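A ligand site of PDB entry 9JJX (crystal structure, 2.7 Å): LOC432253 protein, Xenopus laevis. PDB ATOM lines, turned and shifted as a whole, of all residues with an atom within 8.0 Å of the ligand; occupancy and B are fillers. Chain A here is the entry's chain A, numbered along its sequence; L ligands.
O of Glu 257 is in hydrogen-bond range of OG of Ser 261 (2.7 Å). The backbone carbonyl oxygen of Phe 231 is in hydrogen-bond range of the backbone NH of Val 185. The side-chain hydroxyl (OH) of Tyr 189 sits at hydrogen-bond distance from the side-chain hydroxyl (OG) of Ser 258, 3.4 Å away. The backbone carbonyl oxygen (O) of Asp 254 lies within hydrogen-bond range of the side-chain hydroxyl (OG) of Ser 258, at 3.1 Å. OH of Tyr 189 sits close to O of Lys 193 (3.1 Å).
Residues that only touch the ligand: Phe 231 (3.4 Å). Of the 24 residues printed, 6 come within 4 Å of the ligand.
An oxygen (O4) of the ligand sits at hydrogen-bond distance from the side-chain hydroxyl (OG) of Ser 258 (3.2 Å). O1 of the ligand is in hydrogen-bond range of OG of Ser 261, 3.0 Å away. OH of Tyr 189 is in hydrogen-bond range of O4 of the ligand (3.2 Å). An oxygen (O5) of the ligand sits close to the indole nitrogen (NE1) of Trp 194, 3.4 Å away. An oxygen (O4) of the ligand sits close to the backbone carbonyl oxygen of Leu 232 (2.5 Å).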
ATOM      1  N   LEU A 184     -33.697 -16.982 -12.863  1.00  0.00           N
ATOM      2  CA  LEU A 184     -32.241 -16.991 -12.961  1.00  0.00           C
ATOM      3  C   LEU A 184     -31.849 -17.178 -14.428  1.00  0.00           C
ATOM      4  O   LEU A 184     -32.010 -18.270 -14.982  1.00  0.00           O
ATOM      5  CB  LEU A 184     -31.638 -18.095 -12.086  1.00  0.00           C
ATOM      6  CG  LEU A 184     -30.151 -17.952 -11.763  1.00  0.00           C
ATOM      7  CD1 LEU A 184     -29.922 -16.885 -10.707  1.00  0.00           C
ATOM      8  CD2 LEU A 184     -29.578 -19.292 -11.310  1.00  0.00           C
ATOM      9  N   VAL A 185     -31.342 -16.111 -15.038  1.00  0.00           N
ATOM     10  CA  VAL A 185     -30.880 -16.158 -16.416  1.00  0.00           C
ATOM     11  C   VAL A 185     -29.411 -16.543 -16.409  1.00  0.00           C
ATOM     12  O   VAL A 185     -28.582 -15.888 -15.760  1.00  0.00           O
ATOM     13  CB  VAL A 185     -31.084 -14.801 -17.113  1.00  0.00           C
ATOM     14  CG1 VAL A 185     -31.079 -14.964 -18.627  1.00  0.00           C
ATOM     15  CG2 VAL A 185     -32.380 -14.151 -16.642  1.00  0.00           C
ATOM     16  N   TYR A 189     -24.158 -12.925 -20.044  1.00  0.00           N
ATOM     17  CA  TYR A 189     -23.046 -12.062 -20.394  1.00  0.00           C
ATOM     18  C   TYR A 189     -21.741 -12.742 -20.014  1.00  0.00           C
ATOM     19  O   TYR A 189     -21.732 -13.746 -19.298  1.00  0.00           O
ATOM     20  CB  TYR A 189     -23.180 -10.681 -19.724  1.00  0.00           C
ATOM     21  CG  TYR A 189     -23.034 -10.713 -18.222  1.00  0.00           C
ATOM     22  CD1 TYR A 189     -24.128 -10.926 -17.398  1.00  0.00           C
ATOM     23  CD2 TYR A 189     -21.792 -10.516 -17.619  1.00  0.00           C
ATOM     24  CE1 TYR A 189     -23.998 -10.945 -16.018  1.00  0.00           C
ATOM     25  CE2 TYR A 189     -21.652 -10.532 -16.243  1.00  0.00           C
ATOM     26  CZ  TYR A 189     -22.756 -10.751 -15.448  1.00  0.00           C
ATOM     27  OH  TYR A 189     -22.617 -10.775 -14.083  1.00  0.00           O
ATOM     28  N   SER A 191     -17.853 -11.906 -18.442  1.00  0.00           N
ATOM     29  CA  SER A 191     -17.094 -10.928 -17.667  1.00  0.00           C
ATOM     30  C   SER A 191     -17.898  -9.643 -17.523  1.00  0.00           C
ATOM     31  O   SER A 191     -19.019  -9.656 -17.008  1.00  0.00           O
ATOM     32  CB  SER A 191     -15.733 -10.656 -18.318  1.00  0.00           C
ATOM     33  OG  SER A 191     -15.888 -10.089 -19.601  1.00  0.00           O
ATOM     34  N   LYS A 193     -18.028  -7.632 -15.550  1.00  0.00           N
ATOM     35  CA  LYS A 193     -18.394  -7.425 -14.145  1.00  0.00           C
ATOM     36  C   LYS A 193     -19.910  -7.494 -14.033  1.00  0.00           C
ATOM     37  O   LYS A 193     -20.492  -8.495 -14.492  1.00  0.00           O
ATOM     38  CB  LYS A 193     -17.746  -6.137 -13.641  1.00  0.00           C
ATOM     39  CG  LYS A 193     -17.816  -5.986 -12.135  1.00  0.00           C
ATOM     40  CD  LYS A 193     -17.579  -4.562 -11.684  1.00  0.00           C
ATOM     41  CE  LYS A 193     -17.767  -4.425 -10.177  1.00  0.00           C
ATOM     42  NZ  LYS A 193     -17.844  -3.001  -9.741  1.00  0.00           N
ATOM     43  N   TRP A 194     -20.585  -6.512 -13.440  1.00  0.00           N
ATOM     44  CA  TRP A 194     -22.036  -6.445 -13.499  1.00  0.00           C
ATOM     45  C   TRP A 194     -22.476  -4.989 -13.641  1.00  0.00           C
ATOM     46  O   TRP A 194     -21.878  -4.089 -13.039  1.00  0.00           O
ATOM     47  CB  TRP A 194     -22.710  -7.028 -12.265  1.00  0.00           C
ATOM     48  CG  TRP A 194     -24.180  -7.198 -12.501  1.00  0.00           C
ATOM     49  CD1 TRP A 194     -24.771  -7.708 -13.627  1.00  0.00           C
ATOM     50  CD2 TRP A 194     -25.238  -6.702 -11.680  1.00  0.00           C
ATOM     51  NE1 TRP A 194     -26.141  -7.655 -13.502  1.00  0.00           N
ATOM     52  CE2 TRP A 194     -26.446  -7.029 -12.325  1.00  0.00           C
ATOM     53  CE3 TRP A 194     -25.289  -6.046 -10.448  1.00  0.00           C
ATOM     54  CZ2 TRP A 194     -27.692  -6.712 -11.769  1.00  0.00           C
ATOM     55  CZ3 TRP A 194     -26.525  -5.744  -9.908  1.00  0.00           C
ATOM     56  CH2 TRP A 194     -27.705  -6.073 -10.566  1.00  0.00           C
ATOM     57  N   ASP A 195     -23.546  -4.792 -14.400  1.00  0.00           N
ATOM     58  CA  ASP A 195     -24.229  -3.511 -14.501  1.00  0.00           C
ATOM     59  C   ASP A 195     -25.698  -3.731 -14.136  1.00  0.00           C
ATOM     60  O   ASP A 195     -26.327  -4.669 -14.643  1.00  0.00           O
ATOM     61  CB  ASP A 195     -24.102  -2.931 -15.907  1.00  0.00           C
ATOM     62  CG  ASP A 195     -24.408  -1.436 -15.956  1.00  0.00           C
ATOM     63  OD1 ASP A 195     -24.822  -0.876 -14.918  1.00  0.00           O
ATOM     64  OD2 ASP A 195     -24.248  -0.828 -17.034  1.00  0.00           O
ATOM     65  N   ARG A 196     -26.230  -2.887 -13.261  1.00  0.00           N
ATOM     66  CA  ARG A 196     -27.645  -2.967 -12.909  1.00  0.00           C
ATOM     67  C   ARG A 196     -28.522  -2.553 -14.085  1.00  0.00           C
ATOM     68  O   ARG A 196     -29.744  -2.479 -13.963  1.00  0.00           O
ATOM     69  CB  ARG A 196     -27.961  -2.101 -11.694  1.00  0.00           C
ATOM     70  CG  ARG A 196     -27.283  -2.529 -10.407  1.00  0.00           C
ATOM     71  CD  ARG A 196     -27.841  -1.718  -9.265  1.00  0.00           C
ATOM     72  NE  ARG A 196     -27.808  -0.303  -9.625  1.00  0.00           N
ATOM     73  CZ  ARG A 196     -28.207   0.693  -8.837  1.00  0.00           C
ATOM     74  NH1 ARG A 196     -28.725   0.466  -7.649  1.00  0.00           N
ATOM     75  NH2 ARG A 196     -28.065   1.939  -9.276  1.00  0.00           N
ATOM     76  N   VAL A 198     -28.169  -4.191 -17.335  1.00  0.00           N
ATOM     77  CA  VAL A 198     -28.514  -5.406 -18.071  1.00  0.00           C
ATOM     78  C   VAL A 198     -29.772  -6.048 -17.491  1.00  0.00           C
ATOM     79  O   VAL A 198     -30.657  -6.507 -18.231  1.00  0.00           O
ATOM     80  CB  VAL A 198     -27.337  -6.394 -18.074  1.00  0.00           C
ATOM     81  CG1 VAL A 198     -26.187  -5.836 -18.895  1.00  0.00           C
ATOM     82  CG2 VAL A 198     -26.890  -6.691 -16.654  1.00  0.00           C
ATOM     83  N   ALA A 199     -29.872  -6.093 -16.163  1.00  0.00           N
ATOM     84  CA  ALA A 199     -30.984  -6.790 -15.529  1.00  0.00           C
ATOM     85  C   ALA A 199     -32.308  -6.073 -15.810  1.00  0.00           C
ATOM     86  O   ALA A 199     -33.260  -6.691 -16.316  1.00  0.00           O
ATOM     87  CB  ALA A 199     -30.743  -6.918 -14.025  1.00  0.00           C
ATOM     88  N   CYS A 230     -35.377 -11.074 -10.964  1.00  0.00           N
ATOM     89  CA  CYS A 230     -34.566 -11.662 -12.024  1.00  0.00           C
ATOM     90  C   CYS A 230     -33.089 -11.418 -11.737  1.00  0.00           C
ATOM     91  O   CYS A 230     -32.668 -10.286 -11.500  1.00  0.00           O
ATOM     92  CB  CYS A 230     -34.930 -11.097 -13.397  1.00  0.00           C
ATOM     93  SG  CYS A 230     -36.568 -11.571 -13.977  1.00  0.00           S
ATOM     94  N   PHE A 231     -32.304 -12.495 -11.801  1.00  0.00           N
ATOM     95  CA  PHE A 231     -30.884 -12.496 -11.503  1.00  0.00           C
ATOM     96  C   PHE A 231     -30.147 -13.033 -12.723  1.00  0.00           C
ATOM     97  O   PHE A 231     -30.437 -14.130 -13.182  1.00  0.00           O
ATOM     98  CB  PHE A 231     -30.598 -13.385 -10.296  1.00  0.00           C
ATOM     99  CG  PHE A 231     -29.529 -12.861  -9.393  1.00  0.00           C
ATOM    100  CD1 PHE A 231     -29.722 -11.709  -8.645  1.00  0.00           C
ATOM    101  CD2 PHE A 231     -28.347 -13.567  -9.250  1.00  0.00           C
ATOM    102  CE1 PHE A 231     -28.725 -11.264  -7.789  1.00  0.00           C
ATOM    103  CE2 PHE A 231     -27.350 -13.107  -8.414  1.00  0.00           C
ATOM    104  CZ  PHE A 231     -27.556 -11.989  -7.665  1.00  0.00           C
ATOM    105  N   LEU A 232     -29.181 -12.271 -13.223  1.00  0.00           N
ATOM    106  CA  LEU A 232     -28.454 -12.621 -14.445  1.00  0.00           C
ATOM    107  C   LEU A 232     -26.972 -12.817 -14.102  1.00  0.00           C
ATOM    108  O   LEU A 232     -26.266 -11.840 -13.838  1.00  0.00           O
ATOM    109  CB  LEU A 232     -28.641 -11.564 -15.517  1.00  0.00           C
ATOM    110  CG  LEU A 232     -30.093 -11.201 -15.827  1.00  0.00           C
ATOM    111  CD1 LEU A 232     -30.645 -10.193 -14.813  1.00  0.00           C
ATOM    112  CD2 LEU A 232     -30.226 -10.660 -17.253  1.00  0.00           C
ATOM    113  N   LEU A 233     -26.519 -14.067 -14.121  1.00  0.00           N
ATOM    114  CA  LEU A 233     -25.132 -14.386 -13.833  1.00  0.00           C
ATOM    115  C   LEU A 233     -24.383 -14.706 -15.125  1.00  0.00           C
ATOM    116  O   LEU A 233     -24.983 -15.132 -16.116  1.00  0.00           O
ATOM    117  CB  LEU A 233     -25.021 -15.581 -12.870  1.00  0.00           C
ATOM    118  CG  LEU A 233     -25.809 -16.827 -13.269  1.00  0.00           C
ATOM    119  CD1 LEU A 233     -25.145 -18.079 -12.710  1.00  0.00           C
ATOM    120  CD2 LEU A 233     -27.251 -16.732 -12.794  1.00  0.00           C
ATOM    121  N   PRO A 234     -23.059 -14.500 -15.140  1.00  0.00           N
ATOM    122  CA  PRO A 234     -22.306 -14.703 -16.385  1.00  0.00           C
ATOM    123  C   PRO A 234     -22.099 -16.176 -16.716  1.00  0.00           C
ATOM    124  O   PRO A 234     -22.704 -17.054 -16.105  1.00  0.00           O
ATOM    125  CB  PRO A 234     -20.966 -14.009 -16.089  1.00  0.00           C
ATOM    126  CG  PRO A 234     -20.809 -14.158 -14.619  1.00  0.00           C
ATOM    127  CD  PRO A 234     -22.198 -14.042 -14.043  1.00  0.00           C
ATOM    128  N   ASP A 254     -16.004 -13.331 -11.776  1.00  0.00           N
ATOM    129  CA  ASP A 254     -17.297 -12.668 -11.924  1.00  0.00           C
ATOM    130  C   ASP A 254     -18.440 -13.635 -11.652  1.00  0.00           C
ATOM    131  O   ASP A 254     -19.390 -13.294 -10.929  1.00  0.00           O
ATOM    132  CB  ASP A 254     -17.406 -12.056 -13.317  1.00  0.00           C
ATOM    133  CG  ASP A 254     -16.486 -10.869 -13.512  1.00  0.00           C
ATOM    134  OD1 ASP A 254     -15.857 -10.426 -12.519  1.00  0.00           O
ATOM    135  OD2 ASP A 254     -16.368 -10.381 -14.654  1.00  0.00           O
ATOM    136  N   PHE A 255     -18.363 -14.841 -12.220  1.00  0.00           N
ATOM    137  CA  PHE A 255     -19.356 -15.860 -11.908  1.00  0.00           C
ATOM    138  C   PHE A 255     -19.346 -16.209 -10.427  1.00  0.00           C
ATOM    139  O   PHE A 255     -20.407 -16.388  -9.818  1.00  0.00           O
ATOM    140  CB  PHE A 255     -19.109 -17.117 -12.747  1.00  0.00           C
ATOM    141  CG  PHE A 255     -20.026 -18.259 -12.416  1.00  0.00           C
ATOM    142  CD1 PHE A 255     -21.296 -18.338 -12.970  1.00  0.00           C
ATOM    143  CD2 PHE A 255     -19.620 -19.258 -11.545  1.00  0.00           C
ATOM    144  CE1 PHE A 255     -22.145 -19.390 -12.655  1.00  0.00           C
ATOM    145  CE2 PHE A 255     -20.469 -20.310 -11.229  1.00  0.00           C
ATOM    146  CZ  PHE A 255     -21.722 -20.373 -11.788  1.00  0.00           C
ATOM    147  N   GLU A 257     -18.549 -14.300  -7.831  1.00  0.00           N
ATOM    148  CA  GLU A 257     -19.157 -13.247  -7.027  1.00  0.00           C
ATOM    149  C   GLU A 257     -20.649 -13.143  -7.292  1.00  0.00           C
ATOM    150  O   GLU A 257     -21.436 -12.909  -6.355  1.00  0.00           O
ATOM    151  CB  GLU A 257     -18.464 -11.911  -7.305  1.00  0.00           C
ATOM    152  CG  GLU A 257     -17.081 -11.808  -6.663  1.00  0.00           C
ATOM    153  CD  GLU A 257     -17.029 -12.429  -5.281  1.00  0.00           C
ATOM    154  OE1 GLU A 257     -17.670 -11.879  -4.360  1.00  0.00           O
ATOM    155  OE2 GLU A 257     -16.342 -13.453  -5.113  1.00  0.00           O
ATOM    156  N   SER A 258     -21.083 -13.298  -8.551  1.00  0.00           N
ATOM    157  CA  SER A 258     -22.513 -13.249  -8.838  1.00  0.00           C
ATOM    158  C   SER A 258     -23.248 -14.408  -8.171  1.00  0.00           C
ATOM    159  O   SER A 258     -24.338 -14.233  -7.631  1.00  0.00           O
ATOM    160  CB  SER A 258     -22.741 -13.262 -10.357  1.00  0.00           C
ATOM    161  OG  SER A 258     -22.275 -12.062 -10.943  1.00  0.00           O
ATOM    162  N   LEU A 259     -22.651 -15.604  -8.207  1.00  0.00           N
ATOM    163  CA  LEU A 259     -23.227 -16.746  -7.514  1.00  0.00           C
ATOM    164  C   LEU A 259     -23.318 -16.501  -6.020  1.00  0.00           C
ATOM    165  O   LEU A 259     -24.319 -16.852  -5.383  1.00  0.00           O
ATOM    166  CB  LEU A 259     -22.406 -18.005  -7.803  1.00  0.00           C
ATOM    167  CG  LEU A 259     -23.039 -19.349  -7.430  1.00  0.00           C
ATOM    168  CD1 LEU A 259     -24.060 -19.767  -8.479  1.00  0.00           C
ATOM    169  CD2 LEU A 259     -21.968 -20.416  -7.271  1.00  0.00           C
ATOM    170  N   ARG A 260     -22.275 -15.903  -5.433  1.00  0.00           N
ATOM    171  CA  ARG A 260     -22.320 -15.593  -4.002  1.00  0.00           C
ATOM    172  C   ARG A 260     -23.441 -14.609  -3.697  1.00  0.00           C
ATOM    173  O   ARG A 260     -24.191 -14.803  -2.726  1.00  0.00           O
ATOM    174  CB  ARG A 260     -20.977 -15.050  -3.544  1.00  0.00           C
ATOM    175  CG  ARG A 260     -20.019 -16.127  -3.069  1.00  0.00           C
ATOM    176  CD  ARG A 260     -19.353 -15.749  -1.752  1.00  0.00           C
ATOM    177  NE  ARG A 260     -18.422 -16.781  -1.314  1.00  0.00           N
ATOM    178  CZ  ARG A 260     -17.270 -17.056  -1.913  1.00  0.00           C
ATOM    179  NH1 ARG A 260     -16.861 -16.369  -2.972  1.00  0.00           N
ATOM    180  NH2 ARG A 260     -16.510 -18.027  -1.442  1.00  0.00           N
ATOM    181  N   SER A 261     -23.572 -13.559  -4.498  1.00  0.00           N
ATOM    182  CA  SER A 261     -24.650 -12.594  -4.299  1.00  0.00           C
ATOM    183  C   SER A 261     -26.019 -13.267  -4.385  1.00  0.00           C
ATOM    184  O   SER A 261     -26.899 -13.012  -3.539  1.00  0.00           O
ATOM    185  CB  SER A 261     -24.541 -11.466  -5.317  1.00  0.00           C
ATOM    186  OG  SER A 261     -23.198 -11.011  -5.447  1.00  0.00           O
ATOM    187  N   TYR A 262     -26.220 -14.123  -5.379  1.00  0.00           N
ATOM    188  CA  TYR A 262     -27.524 -14.776  -5.543  1.00  0.00           C
ATOM    189  C   TYR A 262     -27.826 -15.731  -4.402  1.00  0.00           C
ATOM    190  O   TYR A 262     -28.956 -15.783  -3.910  1.00  0.00           O
ATOM    191  CB  TYR A 262     -27.601 -15.522  -6.866  1.00  0.00           C
ATOM    192  CG  TYR A 262     -28.971 -16.113  -7.135  1.00  0.00           C
ATOM    193  CD1 TYR A 262     -30.086 -15.284  -7.299  1.00  0.00           C
ATOM    194  CD2 TYR A 262     -29.151 -17.475  -7.197  1.00  0.00           C
ATOM    195  CE1 TYR A 262     -31.330 -15.815  -7.535  1.00  0.00           C
ATOM    196  CE2 TYR A 262     -30.402 -18.018  -7.432  1.00  0.00           C
ATOM    197  CZ  TYR A 262     -31.486 -17.182  -7.596  1.00  0.00           C
ATOM    198  OH  TYR A 262     -32.728 -17.722  -7.834  1.00  0.00           O
ATOM    199  N   LYS A 265     -28.935 -13.741  -1.559  1.00  0.00           N
ATOM    200  CA  LYS A 265     -30.341 -13.406  -1.794  1.00  0.00           C
ATOM    201  C   LYS A 265     -31.249 -14.534  -1.335  1.00  0.00           C
ATOM    202  O   LYS A 265     -32.205 -14.325  -0.584  1.00  0.00           O
ATOM    203  CB  LYS A 265     -30.572 -13.143  -3.284  1.00  0.00           C
ATOM    204  CG  LYS A 265     -29.640 -12.146  -3.934  1.00  0.00           C
ATOM    205  CD  LYS A 265     -30.177 -10.742  -3.838  1.00  0.00           C
ATOM    206  CE  LYS A 265     -29.551  -9.870  -4.914  1.00  0.00           C
ATOM    207  NZ  LYS A 265     -28.395  -9.098  -4.392  1.00  0.00           N
HETATM  208  C1  LIG L   1     -24.992  -8.360  -7.856  1.00  0.00           C
HETATM  209  O1  LIG L   1     -23.941  -8.739  -7.235  1.00  0.00           O
HETATM  210  O2  LIG L   1     -25.370  -7.172  -7.768  1.00  0.00           O
HETATM  211  C2  LIG L   1     -25.832  -9.263  -8.763  1.00  0.00           C
HETATM  212  O3  LIG L   1     -26.889  -8.566  -9.360  1.00  0.00           O
HETATM  213  C3  LIG L   1     -24.847  -9.857  -9.775  1.00  0.00           C
HETATM  214  C4  LIG L   1     -25.608 -10.225 -11.041  1.00  0.00           C
HETATM  215  O4  LIG L   1     -25.012 -10.753 -12.007  1.00  0.00           O
HETATM  216  O5  LIG L   1     -26.838  -9.985 -11.110  1.00  0.00           O
